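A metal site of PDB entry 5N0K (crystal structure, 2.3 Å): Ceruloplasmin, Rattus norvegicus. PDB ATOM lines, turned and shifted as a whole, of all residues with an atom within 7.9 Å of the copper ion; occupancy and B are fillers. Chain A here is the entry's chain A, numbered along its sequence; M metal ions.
Val 293 touches the copper ion (O to CU, 3.7 Å). Leu 347 touches the copper ion. The nearest printed residue that does not touch the copper ion is Asn 339 (4.1 Å).
N of Cys 337 is in hydrogen-bond range of O of Leu 347 (3.2 Å). N of Asn 339 sits close to SG of Cys 337, at 3.5 Å. NE2 of His 294 lies within hydrogen-bond range of OD2 of Asp 292, 2.8 Å away. N of Leu 347 is in hydrogen-bond range of O of His 342 (3.1 Å). ND2 of Asn 339 is in hydrogen-bond range of NE2 of His 342 (3.1 Å). O of Val 291 lies within hydrogen-bond range of NE2 of His 342 (2.9 Å). A ring nitrogen (NE2) of His 342 sits at hydrogen-bond distance from the side-chain carboxylate (OE1) of Glu 646 (3.3 Å). ND2 of Asn 339 lies within hydrogen-bond range of O of Val 293 (2.9 Å).
The copper ion is bound by SG of Cys 337, ND1 of His 294 and ND1 of His 342. The copper ion has three donor atoms within binding distance.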
ATOM      1  N   PHE A 220       7.405  -0.170  26.364  1.00  0.00           N
ATOM      2  CA  PHE A 220       7.806  -0.065  24.971  1.00  0.00           C
ATOM      3  C   PHE A 220       8.868  -1.074  24.828  1.00  0.00           C
ATOM      4  O   PHE A 220       9.846  -1.027  25.550  1.00  0.00           O
ATOM      5  CB  PHE A 220       8.354   1.328  24.601  1.00  0.00           C
ATOM      6  CG  PHE A 220       7.274   2.345  24.286  1.00  0.00           C
ATOM      7  CD1 PHE A 220       6.289   2.652  25.224  1.00  0.00           C
ATOM      8  CD2 PHE A 220       7.214   2.963  23.049  1.00  0.00           C
ATOM      9  CE1 PHE A 220       5.280   3.557  24.918  1.00  0.00           C
ATOM     10  CE2 PHE A 220       6.219   3.879  22.756  1.00  0.00           C
ATOM     11  CZ  PHE A 220       5.242   4.181  23.691  1.00  0.00           C
ATOM     12  N   SER A 221       8.664  -2.011  23.936  1.00  0.00           N
ATOM     13  CA  SER A 221       9.608  -3.067  23.757  1.00  0.00           C
ATOM     14  C   SER A 221       9.548  -3.688  22.356  1.00  0.00           C
ATOM     15  O   SER A 221       8.460  -3.897  21.818  1.00  0.00           O
ATOM     16  CB  SER A 221       9.371  -4.176  24.779  1.00  0.00           C
ATOM     17  OG  SER A 221      10.445  -5.108  24.735  1.00  0.00           O
ATOM     18  N   VAL A 222      10.724  -3.971  21.807  1.00  0.00           N
ATOM     19  CA  VAL A 222      10.856  -4.840  20.651  1.00  0.00           C
ATOM     20  C   VAL A 222      10.919  -6.257  21.234  1.00  0.00           C
ATOM     21  O   VAL A 222      11.998  -6.821  21.494  1.00  0.00           O
ATOM     22  CB  VAL A 222      12.111  -4.502  19.822  1.00  0.00           C
ATOM     23  CG1 VAL A 222      12.208  -5.410  18.599  1.00  0.00           C
ATOM     24  CG2 VAL A 222      12.082  -3.046  19.378  1.00  0.00           C
ATOM     25  N   TYR A 259       7.320  -5.149  17.521  1.00  0.00           N
ATOM     26  CA  TYR A 259       7.615  -3.793  17.993  1.00  0.00           C
ATOM     27  C   TYR A 259       6.322  -3.241  18.617  1.00  0.00           C
ATOM     28  O   TYR A 259       5.444  -2.756  17.905  1.00  0.00           O
ATOM     29  CB  TYR A 259       8.085  -2.892  16.859  1.00  0.00           C
ATOM     30  CG  TYR A 259       9.434  -3.231  16.233  1.00  0.00           C
ATOM     31  CD1 TYR A 259       9.602  -4.382  15.452  1.00  0.00           C
ATOM     32  CD2 TYR A 259      10.524  -2.363  16.341  1.00  0.00           C
ATOM     33  CE1 TYR A 259      10.810  -4.664  14.835  1.00  0.00           C
ATOM     34  CE2 TYR A 259      11.737  -2.644  15.732  1.00  0.00           C
ATOM     35  CZ  TYR A 259      11.876  -3.803  14.983  1.00  0.00           C
ATOM     36  OH  TYR A 259      13.068  -4.111  14.345  1.00  0.00           O
ATOM     37  N   SER A 260       6.220  -3.316  19.933  1.00  0.00           N
ATOM     38  CA  SER A 260       4.945  -3.257  20.621  1.00  0.00           C
ATOM     39  C   SER A 260       4.950  -2.395  21.871  1.00  0.00           C
ATOM     40  O   SER A 260       6.002  -2.072  22.412  1.00  0.00           O
ATOM     41  CB  SER A 260       4.518  -4.684  21.039  1.00  0.00           C
ATOM     42  OG  SER A 260       5.588  -5.461  21.547  1.00  0.00           O
ATOM     43  N   VAL A 291      18.573  -2.608  20.120  1.00  0.00           N
ATOM     44  CA  VAL A 291      17.572  -1.959  19.230  1.00  0.00           C
ATOM     45  C   VAL A 291      16.496  -1.186  20.000  1.00  0.00           C
ATOM     46  O   VAL A 291      15.828  -0.358  19.405  1.00  0.00           O
ATOM     47  CB  VAL A 291      16.860  -2.909  18.221  1.00  0.00           C
ATOM     48  CG1 VAL A 291      17.819  -3.326  17.127  1.00  0.00           C
ATOM     49  CG2 VAL A 291      16.238  -4.109  18.929  1.00  0.00           C
ATOM     50  N   ASP A 292      16.353  -1.434  21.289  1.00  0.00           N
ATOM     51  CA  ASP A 292      15.368  -0.717  22.107  1.00  0.00           C
ATOM     52  C   ASP A 292      15.741   0.712  22.479  1.00  0.00           C
ATOM     53  O   ASP A 292      15.919   1.034  23.666  1.00  0.00           O
ATOM     54  CB  ASP A 292      15.032  -1.552  23.335  1.00  0.00           C
ATOM     55  CG  ASP A 292      14.247  -2.807  22.956  1.00  0.00           C
ATOM     56  OD1 ASP A 292      14.885  -3.865  22.830  1.00  0.00           O
ATOM     57  OD2 ASP A 292      13.020  -2.694  22.739  1.00  0.00           O
ATOM     58  N   VAL A 293      15.856   1.568  21.437  1.00  0.00           N
ATOM     59  CA  VAL A 293      15.994   2.990  21.541  1.00  0.00           C
ATOM     60  C   VAL A 293      14.626   3.504  21.175  1.00  0.00           C
ATOM     61  O   VAL A 293      14.265   3.528  20.009  1.00  0.00           O
ATOM     62  CB  VAL A 293      17.063   3.519  20.581  1.00  0.00           C
ATOM     63  CG1 VAL A 293      17.144   5.044  20.643  1.00  0.00           C
ATOM     64  CG2 VAL A 293      18.424   2.923  20.943  1.00  0.00           C
ATOM     65  N   HIS A 294      13.848   3.882  22.184  1.00  0.00           N
ATOM     66  CA  HIS A 294      12.479   4.338  21.973  1.00  0.00           C
ATOM     67  C   HIS A 294      12.298   5.814  22.236  1.00  0.00           C
ATOM     68  O   HIS A 294      12.983   6.398  23.075  1.00  0.00           O
ATOM     69  CB  HIS A 294      11.501   3.569  22.869  1.00  0.00           C
ATOM     70  CG  HIS A 294      11.579   2.088  22.697  1.00  0.00           C
ATOM     71  ND1 HIS A 294      11.016   1.434  21.624  1.00  0.00           N
ATOM     72  CD2 HIS A 294      12.185   1.119  23.440  1.00  0.00           C
ATOM     73  CE1 HIS A 294      11.222   0.135  21.734  1.00  0.00           C
ATOM     74  NE2 HIS A 294      11.949  -0.082  22.819  1.00  0.00           N
ATOM     75  N   SER A 295      11.325   6.390  21.521  1.00  0.00           N
ATOM     76  CA  SER A 295      11.006   7.820  21.605  1.00  0.00           C
ATOM     77  C   SER A 295       9.484   7.942  21.551  1.00  0.00           C
ATOM     78  O   SER A 295       8.854   8.149  20.514  1.00  0.00           O
ATOM     79  CB  SER A 295      11.674   8.526  20.426  1.00  0.00           C
ATOM     80  OG  SER A 295      13.112   8.528  20.585  1.00  0.00           O
ATOM     81  N   ALA A 296       8.874   7.772  22.706  1.00  0.00           N
ATOM     82  CA  ALA A 296       7.418   7.898  22.850  1.00  0.00           C
ATOM     83  C   ALA A 296       6.895   9.294  22.637  1.00  0.00           C
ATOM     84  O   ALA A 296       7.313  10.215  23.348  1.00  0.00           O
ATOM     85  CB  ALA A 296       6.989   7.412  24.220  1.00  0.00           C
ATOM     86  N   ILE A 313       9.325  11.060  25.294  1.00  0.00           N
ATOM     87  CA  ILE A 313       9.825  10.246  26.391  1.00  0.00           C
ATOM     88  C   ILE A 313      10.693   9.140  25.801  1.00  0.00           C
ATOM     89  O   ILE A 313      10.187   8.260  25.093  1.00  0.00           O
ATOM     90  CB  ILE A 313       8.695   9.642  27.259  1.00  0.00           C
ATOM     91  CG1 ILE A 313       7.953  10.747  28.044  1.00  0.00           C
ATOM     92  CG2 ILE A 313       9.270   8.672  28.275  1.00  0.00           C
ATOM     93  CD1 ILE A 313       6.847  11.404  27.245  1.00  0.00           C
ATOM     94  N   LEU A 315      13.116   5.849  26.102  1.00  0.00           N
ATOM     95  CA  LEU A 315      13.035   4.649  26.931  1.00  0.00           C
ATOM     96  C   LEU A 315      14.018   3.691  26.362  1.00  0.00           C
ATOM     97  O   LEU A 315      14.071   3.534  25.166  1.00  0.00           O
ATOM     98  CB  LEU A 315      11.646   4.016  26.878  1.00  0.00           C
ATOM     99  CG  LEU A 315      10.499   4.878  27.413  1.00  0.00           C
ATOM    100  CD1 LEU A 315       9.201   4.254  27.035  1.00  0.00           C
ATOM    101  CD2 LEU A 315      10.570   5.114  28.923  1.00  0.00           C
ATOM    102  N   SER A 336       2.987   6.927  19.426  1.00  0.00           N
ATOM    103  CA  SER A 336       3.919   6.254  18.550  1.00  0.00           C
ATOM    104  C   SER A 336       5.353   6.381  19.073  1.00  0.00           C
ATOM    105  O   SER A 336       5.645   7.225  19.902  1.00  0.00           O
ATOM    106  CB  SER A 336       3.855   6.878  17.171  1.00  0.00           C
ATOM    107  OG  SER A 336       4.112   8.259  17.279  1.00  0.00           O
ATOM    108  N   CYS A 337       6.208   5.484  18.635  1.00  0.00           N
ATOM    109  CA  CYS A 337       7.645   5.640  18.814  1.00  0.00           C
ATOM    110  C   CYS A 337       8.148   6.367  17.570  1.00  0.00           C
ATOM    111  O   CYS A 337       7.852   5.968  16.461  1.00  0.00           O
ATOM    112  CB  CYS A 337       8.313   4.283  18.998  1.00  0.00           C
ATOM    113  SG  CYS A 337      10.088   4.385  19.162  1.00  0.00           S
ATOM    114  N   GLN A 338       8.911   7.439  17.767  1.00  0.00           N
ATOM    115  CA  GLN A 338       9.478   8.220  16.676  1.00  0.00           C
ATOM    116  C   GLN A 338      10.829   7.750  16.205  1.00  0.00           C
ATOM    117  O   GLN A 338      11.427   8.371  15.338  1.00  0.00           O
ATOM    118  CB  GLN A 338       9.572   9.682  17.102  1.00  0.00           C
ATOM    119  CG  GLN A 338       8.235  10.317  17.427  1.00  0.00           C
ATOM    120  CD  GLN A 338       7.368  10.466  16.191  1.00  0.00           C
ATOM    121  OE1 GLN A 338       7.507  11.425  15.440  1.00  0.00           O
ATOM    122  NE2 GLN A 338       6.489   9.539  15.982  1.00  0.00           N
ATOM    123  N   ASN A 339      11.354   6.678  16.802  1.00  0.00           N
ATOM    124  CA  ASN A 339      12.426   5.904  16.179  1.00  0.00           C
ATOM    125  C   ASN A 339      11.829   5.424  14.857  1.00  0.00           C
ATOM    126  O   ASN A 339      10.955   4.564  14.850  1.00  0.00           O
ATOM    127  CB  ASN A 339      12.852   4.726  17.039  1.00  0.00           C
ATOM    128  CG  ASN A 339      13.872   3.821  16.365  1.00  0.00           C
ATOM    129  OD1 ASN A 339      13.861   3.639  15.155  1.00  0.00           O
ATOM    130  ND2 ASN A 339      14.759   3.221  17.175  1.00  0.00           N
ATOM    131  N   LEU A 340      12.339   5.999  13.755  1.00  0.00           N
ATOM    132  CA  LEU A 340      11.766   5.781  12.431  1.00  0.00           C
ATOM    133  C   LEU A 340      11.756   4.297  12.016  1.00  0.00           C
ATOM    134  O   LEU A 340      10.805   3.861  11.334  1.00  0.00           O
ATOM    135  CB  LEU A 340      12.525   6.599  11.403  1.00  0.00           C
ATOM    136  CG  LEU A 340      12.473   8.110  11.637  1.00  0.00           C
ATOM    137  CD1 LEU A 340      13.268   8.762  10.519  1.00  0.00           C
ATOM    138  CD2 LEU A 340      11.065   8.636  11.739  1.00  0.00           C
ATOM    139  N   ASN A 341      12.756   3.522  12.436  1.00  0.00           N
ATOM    140  CA  ASN A 341      12.694   2.076  12.227  1.00  0.00           C
ATOM    141  C   ASN A 341      11.602   1.386  13.002  1.00  0.00           C
ATOM    142  O   ASN A 341      11.018   0.442  12.488  1.00  0.00           O
ATOM    143  CB  ASN A 341      14.002   1.391  12.530  1.00  0.00           C
ATOM    144  CG  ASN A 341      15.049   1.621  11.445  1.00  0.00           C
ATOM    145  OD1 ASN A 341      14.767   2.091  10.365  1.00  0.00           O
ATOM    146  ND2 ASN A 341      16.273   1.331  11.768  1.00  0.00           N
ATOM    147  N   HIS A 342      11.326   1.856  14.214  1.00  0.00           N
ATOM    148  CA  HIS A 342      10.299   1.272  15.049  1.00  0.00           C
ATOM    149  C   HIS A 342       8.904   1.610  14.587  1.00  0.00           C
ATOM    150  O   HIS A 342       8.012   0.767  14.623  1.00  0.00           O
ATOM    151  CB  HIS A 342      10.476   1.698  16.505  1.00  0.00           C
ATOM    152  CG  HIS A 342      11.708   1.170  17.142  1.00  0.00           C
ATOM    153  ND1 HIS A 342      11.868   1.122  18.489  1.00  0.00           N
ATOM    154  CD2 HIS A 342      12.841   0.670  16.599  1.00  0.00           C
ATOM    155  CE1 HIS A 342      13.065   0.649  18.778  1.00  0.00           C
ATOM    156  NE2 HIS A 342      13.661   0.338  17.657  1.00  0.00           N
ATOM    157  N   LEU A 343       8.719   2.863  14.171  1.00  0.00           N
ATOM    158  CA  LEU A 343       7.447   3.366  13.697  1.00  0.00           C
ATOM    159  C   LEU A 343       6.937   2.550  12.535  1.00  0.00           C
ATOM    160  O   LEU A 343       5.826   2.051  12.580  1.00  0.00           O
ATOM    161  CB  LEU A 343       7.613   4.810  13.263  1.00  0.00           C
ATOM    162  CG  LEU A 343       6.382   5.551  12.853  1.00  0.00           C
ATOM    163  CD1 LEU A 343       5.502   5.821  14.042  1.00  0.00           C
ATOM    164  CD2 LEU A 343       6.859   6.873  12.313  1.00  0.00           C
ATOM    165  N   LEU A 347       5.191   0.034  15.783  1.00  0.00           N
ATOM    166  CA  LEU A 347       5.147   0.510  17.181  1.00  0.00           C
ATOM    167  C   LEU A 347       4.349   1.825  17.316  1.00  0.00           C
ATOM    168  O   LEU A 347       4.880   2.958  17.291  1.00  0.00           O
ATOM    169  CB  LEU A 347       6.538   0.662  17.739  1.00  0.00           C
ATOM    170  CG  LEU A 347       6.643   0.358  19.227  1.00  0.00           C
ATOM    171  CD1 LEU A 347       8.138   0.420  19.543  1.00  0.00           C
ATOM    172  CD2 LEU A 347       5.818   1.345  20.062  1.00  0.00           C
ATOM    173  N   GLU A 646      17.600   3.908  15.782  1.00  0.00           N
ATOM    174  CA  GLU A 646      18.464   3.450  16.870  1.00  0.00           C
ATOM    175  C   GLU A 646      19.959   3.782  16.717  1.00  0.00           C
ATOM    176  O   GLU A 646      20.691   3.822  17.718  1.00  0.00           O
ATOM    177  CB  GLU A 646      18.239   1.975  17.180  1.00  0.00           C
ATOM    178  CG  GLU A 646      18.501   0.981  16.035  1.00  0.00           C
ATOM    179  CD  GLU A 646      17.310   0.772  15.094  1.00  0.00           C
ATOM    180  OE1 GLU A 646      16.114   0.903  15.478  1.00  0.00           O
ATOM    181  OE2 GLU A 646      17.591   0.479  13.932  1.00  0.00           O
HETATM  182 CU    CU M   1      10.718   2.484  19.779  1.00  0.00          CU
